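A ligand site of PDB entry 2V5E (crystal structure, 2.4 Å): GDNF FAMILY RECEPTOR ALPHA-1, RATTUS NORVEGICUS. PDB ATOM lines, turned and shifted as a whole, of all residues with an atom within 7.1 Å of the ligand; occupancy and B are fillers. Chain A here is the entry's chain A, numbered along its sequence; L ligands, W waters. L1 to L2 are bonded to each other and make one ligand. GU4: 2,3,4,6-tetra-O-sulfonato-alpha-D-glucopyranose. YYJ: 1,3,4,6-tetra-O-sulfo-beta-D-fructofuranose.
NZ of Lys 45 lies within salt-bridge range of O27 of GU4 L1 (2.7 Å).
The side-chain amide nitrogen (NE2) of Gln 49 is in hydrogen-bond range of an oxygen (O3S3) of YYJ L2 (2.7 Å).
O1S3 of YYJ L2 lies within salt-bridge range of NE of Arg 48, at 2.7 Å.
The side-chain amide nitrogen (ND2) of Asn 104 sits at hydrogen-bond distance from an oxygen (O26) of GU4 L1.
The side-chain amino group (NZ) of Lys 53 is in salt-bridge range of an oxygen (O3S4) of YYJ L2 (3.0 Å).
The guanidinium group of Arg 41 is in salt-bridge range of an oxygen (O28) of GU4 L1, at 3.0 Å.
The backbone NH (N) of Ile 106 sits at hydrogen-bond distance from an oxygen (O23) of GU4 L1 (3.5 Å).
NH1 of Arg 48 sits at hydrogen-bond distance from O of Gly 145 (2.9 Å).
N of Ile 106 sits at hydrogen-bond distance from OD1 of Asn 104, 3.2 Å away.
OD1 of Asn 104 lies within hydrogen-bond range of N of Cys 107 (2.9 Å).
CB of Tyr 105 touches O23 of GU4 L1 (3.3 Å).
Hydrophobic or aromatic side chains that line the ligand: Tyr 105 and Ile 106.
Eight residues have an atom within 4 Å of the ligand: Arg 41, Lys 45, Arg 48, Gln 49, Lys 53, Asn 104, Tyr 105 and Ile 106.
Water W7 bridges an oxygen (O22) of GU4 L1 (2.8 Å) and the backbone NH of Tyr 105 (3.1 Å).
Water W5 bridges O2S4 of YYJ L2 (2.8 Å) and NZ of Lys 53 (3.0 Å).
Water W3 lies within hydrogen-bond range of OD1 of Asn 104 (2.6 Å) and O24 of GU4 L1 (3.1 Å).
Water W1 lies within hydrogen-bond range of the backbone carbonyl oxygen of Arg 41, the guanidinium group of Arg 48 and an oxygen (O29) of GU4 L1.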
ATOM      1  N   ARG A  41      -4.635  14.550  -4.192  1.00  0.00           N
ATOM      2  CA  ARG A  41      -5.680  13.569  -3.886  1.00  0.00           C
ATOM      3  C   ARG A  41      -7.080  14.095  -4.222  1.00  0.00           C
ATOM      4  O   ARG A  41      -7.875  13.412  -4.870  1.00  0.00           O
ATOM      5  CB  ARG A  41      -5.604  13.100  -2.422  1.00  0.00           C
ATOM      6  CG  ARG A  41      -6.770  12.188  -1.995  1.00  0.00           C
ATOM      7  CD  ARG A  41      -6.682  11.678  -0.554  1.00  0.00           C
ATOM      8  NE  ARG A  41      -7.273  12.597   0.417  1.00  0.00           N
ATOM      9  CZ  ARG A  41      -8.492  13.117   0.305  1.00  0.00           C
ATOM     10  NH1 ARG A  41      -9.241  12.843  -0.742  1.00  0.00           N
ATOM     11  NH2 ARG A  41      -8.944  13.942   1.233  1.00  0.00           N
ATOM     12  N   LYS A  42      -7.398  15.299  -3.764  1.00  0.00           N
ATOM     13  CA  LYS A  42      -8.728  15.920  -3.975  1.00  0.00           C
ATOM     14  C   LYS A  42      -8.937  16.294  -5.445  1.00  0.00           C
ATOM     15  O   LYS A  42     -10.051  16.234  -5.956  1.00  0.00           O
ATOM     16  CB  LYS A  42      -8.895  17.180  -3.131  1.00  0.00           C
ATOM     17  CG  LYS A  42      -9.014  16.953  -1.629  1.00  0.00           C
ATOM     18  CD  LYS A  42      -9.459  18.256  -0.927  1.00  0.00           C
ATOM     19  CE  LYS A  42      -9.750  18.024   0.567  1.00  0.00           C
ATOM     20  NZ  LYS A  42     -10.081  19.300   1.289  1.00  0.00           N
ATOM     21  N   HIS A  44      -7.391  14.658  -8.022  1.00  0.00           N
ATOM     22  CA  HIS A  44      -7.607  13.319  -8.591  1.00  0.00           C
ATOM     23  C   HIS A  44      -9.043  12.823  -8.410  1.00  0.00           C
ATOM     24  O   HIS A  44      -9.693  12.420  -9.386  1.00  0.00           O
ATOM     25  CB  HIS A  44      -6.571  12.328  -8.043  1.00  0.00           C
ATOM     26  CG  HIS A  44      -5.256  12.365  -8.766  1.00  0.00           C
ATOM     27  ND1 HIS A  44      -4.222  11.491  -8.476  1.00  0.00           N
ATOM     28  CD2 HIS A  44      -4.818  13.144  -9.793  1.00  0.00           C
ATOM     29  CE1 HIS A  44      -3.202  11.738  -9.295  1.00  0.00           C
ATOM     30  NE2 HIS A  44      -3.535  12.729 -10.093  1.00  0.00           N
ATOM     31  N   LYS A  45      -9.545  12.918  -7.186  1.00  0.00           N
ATOM     32  CA  LYS A  45     -10.925  12.517  -6.887  1.00  0.00           C
ATOM     33  C   LYS A  45     -11.942  13.192  -7.798  1.00  0.00           C
ATOM     34  O   LYS A  45     -12.763  12.522  -8.432  1.00  0.00           O
ATOM     35  CB  LYS A  45     -11.255  12.810  -5.419  1.00  0.00           C
ATOM     36  CG  LYS A  45     -12.506  12.147  -4.893  1.00  0.00           C
ATOM     37  CD  LYS A  45     -12.683  12.493  -3.430  1.00  0.00           C
ATOM     38  CE  LYS A  45     -14.046  12.082  -2.902  1.00  0.00           C
ATOM     39  NZ  LYS A  45     -14.096  10.631  -2.630  1.00  0.00           N
ATOM     40  N   ALA A  46     -11.870  14.515  -7.886  1.00  0.00           N
ATOM     41  CA  ALA A  46     -12.809  15.279  -8.682  1.00  0.00           C
ATOM     42  C   ALA A  46     -12.682  14.954 -10.175  1.00  0.00           C
ATOM     43  O   ALA A  46     -13.683  14.935 -10.901  1.00  0.00           O
ATOM     44  CB  ALA A  46     -12.642  16.758  -8.416  1.00  0.00           C
ATOM     45  N   LEU A  47     -11.449  14.665 -10.627  1.00  0.00           N
ATOM     46  CA  LEU A  47     -11.231  14.231 -12.019  1.00  0.00           C
ATOM     47  C   LEU A  47     -11.938  12.912 -12.336  1.00  0.00           C
ATOM     48  O   LEU A  47     -12.588  12.802 -13.373  1.00  0.00           O
ATOM     49  CB  LEU A  47      -9.734  14.148 -12.354  1.00  0.00           C
ATOM     50  CG  LEU A  47      -9.040  15.490 -12.674  1.00  0.00           C
ATOM     51  CD1 LEU A  47      -7.535  15.343 -12.539  1.00  0.00           C
ATOM     52  CD2 LEU A  47      -9.391  15.976 -14.060  1.00  0.00           C
ATOM     53  N   ARG A  48     -11.792  11.939 -11.440  1.00  0.00           N
ATOM     54  CA  ARG A  48     -12.469  10.640 -11.565  1.00  0.00           C
ATOM     55  C   ARG A  48     -13.982  10.833 -11.624  1.00  0.00           C
ATOM     56  O   ARG A  48     -14.645  10.320 -12.525  1.00  0.00           O
ATOM     57  CB  ARG A  48     -12.093   9.697 -10.414  1.00  0.00           C
ATOM     58  CG  ARG A  48     -10.665   9.154 -10.466  1.00  0.00           C
ATOM     59  CD  ARG A  48     -10.443   7.968  -9.507  1.00  0.00           C
ATOM     60  NE  ARG A  48     -10.921   8.249  -8.153  1.00  0.00           N
ATOM     61  CZ  ARG A  48     -10.194   8.803  -7.188  1.00  0.00           C
ATOM     62  NH1 ARG A  48      -8.933   9.154  -7.396  1.00  0.00           N
ATOM     63  NH2 ARG A  48     -10.744   8.996  -5.984  1.00  0.00           N
ATOM     64  N   GLN A  49     -14.519  11.612 -10.669  1.00  0.00           N
ATOM     65  CA  GLN A  49     -15.952  11.931 -10.669  1.00  0.00           C
ATOM     66  C   GLN A  49     -16.402  12.630 -11.942  1.00  0.00           C
ATOM     67  O   GLN A  49     -17.479  12.315 -12.449  1.00  0.00           O
ATOM     68  CB  GLN A  49     -16.351  12.742  -9.419  1.00  0.00           C
ATOM     69  CG  GLN A  49     -15.963  12.046  -8.091  1.00  0.00           C
ATOM     70  CD  GLN A  49     -16.652  12.625  -6.858  1.00  0.00           C
ATOM     71  OE1 GLN A  49     -17.021  13.796  -6.812  1.00  0.00           O
ATOM     72  NE2 GLN A  49     -16.835  11.788  -5.845  1.00  0.00           N
ATOM     73  N   ASP A  52     -16.521   9.810 -14.608  1.00  0.00           N
ATOM     74  CA  ASP A  52     -17.505   8.792 -14.231  1.00  0.00           C
ATOM     75  C   ASP A  52     -18.932   9.333 -14.267  1.00  0.00           C
ATOM     76  O   ASP A  52     -19.854   8.603 -14.596  1.00  0.00           O
ATOM     77  CB  ASP A  52     -17.187   8.233 -12.830  1.00  0.00           C
ATOM     78  CG  ASP A  52     -17.980   6.967 -12.497  1.00  0.00           C
ATOM     79  OD1 ASP A  52     -18.050   6.026 -13.335  1.00  0.00           O
ATOM     80  OD2 ASP A  52     -18.511   6.916 -11.366  1.00  0.00           O
ATOM     81  N   LYS A  53     -19.106  10.617 -13.959  1.00  0.00           N
ATOM     82  CA  LYS A  53     -20.455  11.165 -13.796  1.00  0.00           C
ATOM     83  C   LYS A  53     -20.958  11.944 -14.991  1.00  0.00           C
ATOM     84  O   LYS A  53     -22.162  12.085 -15.155  1.00  0.00           O
ATOM     85  CB  LYS A  53     -20.574  11.974 -12.507  1.00  0.00           C
ATOM     86  CG  LYS A  53     -20.622  11.128 -11.230  1.00  0.00           C
ATOM     87  CD  LYS A  53     -21.550   9.904 -11.422  1.00  0.00           C
ATOM     88  CE  LYS A  53     -22.164   9.391 -10.121  1.00  0.00           C
ATOM     89  NZ  LYS A  53     -21.156   9.085  -9.106  1.00  0.00           N
ATOM     90  N   THR A 103      -1.687  -1.718  -6.274  1.00  0.00           N
ATOM     91  CA  THR A 103      -2.144  -1.843  -4.874  1.00  0.00           C
ATOM     92  C   THR A 103      -3.489  -1.128  -4.644  1.00  0.00           C
ATOM     93  O   THR A 103      -4.067  -1.199  -3.561  1.00  0.00           O
ATOM     94  CB  THR A 103      -1.124  -1.262  -3.860  1.00  0.00           C
ATOM     95  OG1 THR A 103      -1.077   0.168  -3.987  1.00  0.00           O
ATOM     96  CG2 THR A 103       0.300  -1.862  -4.079  1.00  0.00           C
ATOM     97  N   ASN A 104      -3.981  -0.441  -5.672  1.00  0.00           N
ATOM     98  CA  ASN A 104      -5.207   0.317  -5.557  1.00  0.00           C
ATOM     99  C   ASN A 104      -6.266  -0.291  -6.449  1.00  0.00           C
ATOM    100  O   ASN A 104      -6.021  -0.535  -7.641  1.00  0.00           O
ATOM    101  CB  ASN A 104      -4.986   1.791  -5.932  1.00  0.00           C
ATOM    102  CG  ASN A 104      -6.261   2.593  -5.886  1.00  0.00           C
ATOM    103  OD1 ASN A 104      -6.885   2.866  -6.924  1.00  0.00           O
ATOM    104  ND2 ASN A 104      -6.691   2.931  -4.675  1.00  0.00           N
ATOM    105  N   TYR A 105      -7.447  -0.544  -5.882  1.00  0.00           N
ATOM    106  CA  TYR A 105      -8.479  -1.264  -6.624  1.00  0.00           C
ATOM    107  C   TYR A 105      -8.828  -0.554  -7.940  1.00  0.00           C
ATOM    108  O   TYR A 105      -8.865  -1.187  -8.992  1.00  0.00           O
ATOM    109  CB  TYR A 105      -9.736  -1.538  -5.787  1.00  0.00           C
ATOM    110  CG  TYR A 105     -10.926  -1.824  -6.665  1.00  0.00           C
ATOM    111  CD1 TYR A 105     -11.016  -3.025  -7.390  1.00  0.00           C
ATOM    112  CD2 TYR A 105     -11.962  -0.894  -6.801  1.00  0.00           C
ATOM    113  CE1 TYR A 105     -12.084  -3.289  -8.226  1.00  0.00           C
ATOM    114  CE2 TYR A 105     -13.034  -1.151  -7.642  1.00  0.00           C
ATOM    115  CZ  TYR A 105     -13.093  -2.352  -8.352  1.00  0.00           C
ATOM    116  OH  TYR A 105     -14.172  -2.631  -9.166  1.00  0.00           O
ATOM    117  N   ILE A 106      -9.092   0.753  -7.872  1.00  0.00           N
ATOM    118  CA  ILE A 106      -9.516   1.485  -9.070  1.00  0.00           C
ATOM    119  C   ILE A 106      -8.375   1.539 -10.108  1.00  0.00           C
ATOM    120  O   ILE A 106      -8.589   1.262 -11.296  1.00  0.00           O
ATOM    121  CB  ILE A 106      -9.946   2.931  -8.721  1.00  0.00           C
ATOM    122  CG1 ILE A 106     -11.282   2.949  -7.969  1.00  0.00           C
ATOM    123  CG2 ILE A 106      -9.993   3.796 -10.004  1.00  0.00           C
ATOM    124  CD1 ILE A 106     -11.710   4.334  -7.512  1.00  0.00           C
ATOM    125  N   CYS A 107      -7.176   1.872  -9.648  1.00  0.00           N
ATOM    126  CA  CYS A 107      -6.041   1.942 -10.563  1.00  0.00           C
ATOM    127  C   CYS A 107      -5.766   0.591 -11.227  1.00  0.00           C
ATOM    128  O   CYS A 107      -5.696   0.507 -12.459  1.00  0.00           O
ATOM    129  CB  CYS A 107      -4.777   2.494  -9.890  1.00  0.00           C
ATOM    130  SG  CYS A 107      -3.603   3.138 -11.117  1.00  0.00           S
ATOM    131  N   ARG A 110      -8.624  -0.081 -13.837  1.00  0.00           N
ATOM    132  CA  ARG A 110      -8.525   0.824 -14.987  1.00  0.00           C
ATOM    133  C   ARG A 110      -7.273   0.532 -15.839  1.00  0.00           C
ATOM    134  O   ARG A 110      -7.329   0.516 -17.068  1.00  0.00           O
ATOM    135  CB  ARG A 110      -8.527   2.289 -14.524  1.00  0.00           C
ATOM    136  CG  ARG A 110      -9.744   2.717 -13.677  1.00  0.00           C
ATOM    137  CD  ARG A 110     -11.002   2.864 -14.472  1.00  0.00           C
ATOM    138  NE  ARG A 110     -12.164   3.210 -13.656  1.00  0.00           N
ATOM    139  CZ  ARG A 110     -12.547   4.445 -13.323  1.00  0.00           C
ATOM    140  NH1 ARG A 110     -11.859   5.513 -13.704  1.00  0.00           N
ATOM    141  NH2 ARG A 110     -13.635   4.627 -12.598  1.00  0.00           N
ATOM    142  N   GLY A 145      -6.923  10.687 -12.897  1.00  0.00           N
ATOM    143  CA  GLY A 145      -7.247  10.699 -11.489  1.00  0.00           C
ATOM    144  C   GLY A 145      -6.708   9.488 -10.725  1.00  0.00           C
ATOM    145  O   GLY A 145      -7.005   9.327  -9.543  1.00  0.00           O
ATOM    146  N   THR A 146      -5.945   8.631 -11.400  1.00  0.00           N
ATOM    147  CA  THR A 146      -5.218   7.554 -10.696  1.00  0.00           C
ATOM    148  C   THR A 146      -3.752   7.957 -10.673  1.00  0.00           C
ATOM    149  O   THR A 146      -3.391   8.923 -11.328  1.00  0.00           O
ATOM    150  CB  THR A 146      -5.372   6.187 -11.387  1.00  0.00           C
ATOM    151  OG1 THR A 146      -4.625   6.183 -12.606  1.00  0.00           O
ATOM    152  CG2 THR A 146      -6.841   5.882 -11.691  1.00  0.00           C
HETATM  153  C1  GU4 L   1     -14.034   5.968  -2.197  1.00  0.00           C
HETATM  154  O5  GU4 L   1     -13.369   4.810  -2.697  1.00  0.00           O
HETATM  155  C5  GU4 L   1     -12.315   5.149  -3.658  1.00  0.00           C
HETATM  156  C6  GU4 L   1     -11.747   3.855  -4.184  1.00  0.00           C
HETATM  157  O6  GU4 L   1     -11.226   3.048  -3.134  1.00  0.00           O
HETATM  158  S6  GU4 L   1     -10.918   1.651  -3.387  1.00  0.00           S
HETATM  159  O22 GU4 L   1     -10.241   1.073  -2.163  1.00  0.00           O
HETATM  160  O23 GU4 L   1      -9.978   1.559  -4.589  1.00  0.00           O
HETATM  161  O21 GU4 L   1     -12.207   0.877  -3.712  1.00  0.00           O
HETATM  162  C4  GU4 L   1     -11.226   6.023  -3.011  1.00  0.00           C
HETATM  163  O4  GU4 L   1     -10.313   6.509  -4.014  1.00  0.00           O
HETATM  164  S4  GU4 L   1      -8.921   6.112  -4.035  1.00  0.00           S
HETATM  165  O25 GU4 L   1      -8.268   6.320  -2.677  1.00  0.00           O
HETATM  166  O26 GU4 L   1      -8.814   4.651  -4.401  1.00  0.00           O
HETATM  167  O24 GU4 L   1      -8.214   6.928  -5.103  1.00  0.00           O
HETATM  168  C3  GU4 L   1     -11.867   7.253  -2.370  1.00  0.00           C
HETATM  169  O3  GU4 L   1     -10.820   8.013  -1.706  1.00  0.00           O
HETATM  170  S3  GU4 L   1     -10.661   9.482  -1.850  1.00  0.00           S
HETATM  171  O28 GU4 L   1      -9.414   9.874  -1.094  1.00  0.00           O
HETATM  172  O29 GU4 L   1     -10.548   9.878  -3.327  1.00  0.00           O
HETATM  173  O27 GU4 L   1     -11.864  10.218  -1.255  1.00  0.00           O
HETATM  174  C2  GU4 L   1     -13.017   6.842  -1.426  1.00  0.00           C
HETATM  175  O2  GU4 L   1     -13.712   8.006  -0.919  1.00  0.00           O
HETATM  176  S2  GU4 L   1     -14.201   8.072   0.481  1.00  0.00           S
HETATM  177  O11 GU4 L   1     -13.012   7.887   1.422  1.00  0.00           O
HETATM  178  O12 GU4 L   1     -14.871   9.418   0.727  1.00  0.00           O
HETATM  179  O10 GU4 L   1     -15.209   6.967   0.716  1.00  0.00           O
HETATM  180  C1  YYJ L   2     -16.953   7.112  -2.607  1.00  0.00           C
HETATM  181  C2  YYJ L   2     -15.995   6.497  -3.669  1.00  0.00           C
HETATM  182  C3  YYJ L   2     -16.281   7.134  -5.044  1.00  0.00           C
HETATM  183  C4  YYJ L   2     -17.250   6.164  -5.707  1.00  0.00           C
HETATM  184  C5  YYJ L   2     -16.808   4.819  -5.168  1.00  0.00           C
HETATM  185  C6  YYJ L   2     -15.840   4.210  -6.211  1.00  0.00           C
HETATM  186  O1  YYJ L   2     -16.689   8.524  -2.377  1.00  0.00           O
HETATM  187 O1S1 YYJ L   2     -18.213   9.047  -0.518  1.00  0.00           O
HETATM  188 O1S3 YYJ L   2     -13.556   8.285  -7.410  1.00  0.00           O
HETATM  189 O1S4 YYJ L   2     -19.725   5.446  -7.267  1.00  0.00           O
HETATM  190 O1S6 YYJ L   2     -15.957   1.569  -7.671  1.00  0.00           O
HETATM  191  O2  YYJ L   2     -14.604   6.700  -3.328  1.00  0.00           O
HETATM  192 O2S1 YYJ L   2     -17.151  10.860  -1.831  1.00  0.00           O
HETATM  193 O2S3 YYJ L   2     -13.325   8.604  -4.956  1.00  0.00           O
HETATM  194 O2S4 YYJ L   2     -20.951   6.637  -5.467  1.00  0.00           O
HETATM  195 O2S6 YYJ L   2     -15.192   0.637  -5.455  1.00  0.00           O
HETATM  196  O3  YYJ L   2     -15.075   7.207  -5.845  1.00  0.00           O
HETATM  197 O3S1 YYJ L   2     -18.929   9.441  -2.865  1.00  0.00           O
HETATM  198 O3S3 YYJ L   2     -15.237   9.637  -6.110  1.00  0.00           O
HETATM  199 O3S4 YYJ L   2     -19.456   7.863  -7.022  1.00  0.00           O
HETATM  200 O3S6 YYJ L   2     -17.412   1.699  -5.693  1.00  0.00           O
HETATM  201  O4  YYJ L   2     -18.591   6.382  -5.297  1.00  0.00           O
HETATM  202  O5  YYJ L   2     -16.206   5.077  -3.838  1.00  0.00           O
HETATM  203  O6  YYJ L   2     -15.344   2.956  -5.776  1.00  0.00           O
HETATM  204  S1  YYJ L   2     -17.745   9.455  -1.914  1.00  0.00           S
HETATM  205  S3  YYJ L   2     -14.312   8.426  -6.085  1.00  0.00           S
HETATM  206  S4  YYJ L   2     -19.653   6.570  -6.255  1.00  0.00           S
HETATM  207  S6  YYJ L   2     -15.965   1.734  -6.158  1.00  0.00           S
HETATM  208  O   HOH W   1      -7.664  10.723  -4.949  1.00  0.00           O
HETATM  209  O   HOH W   2     -19.354   6.627  -0.839  1.00  0.00           O
HETATM  210  O   HOH W   3      -7.235   5.402  -7.591  1.00  0.00           O
HETATM  211  O   HOH W   4     -11.972  -1.689  -2.900  1.00  0.00           O
HETATM  212  O   HOH W   5     -22.866   8.252  -6.814  1.00  0.00           O
HETATM  213  O   HOH W   6     -21.002   7.190  -2.884  1.00  0.00           O
HETATM  214  O   HOH W   7      -7.808  -0.141  -2.819  1.00  0.00           O
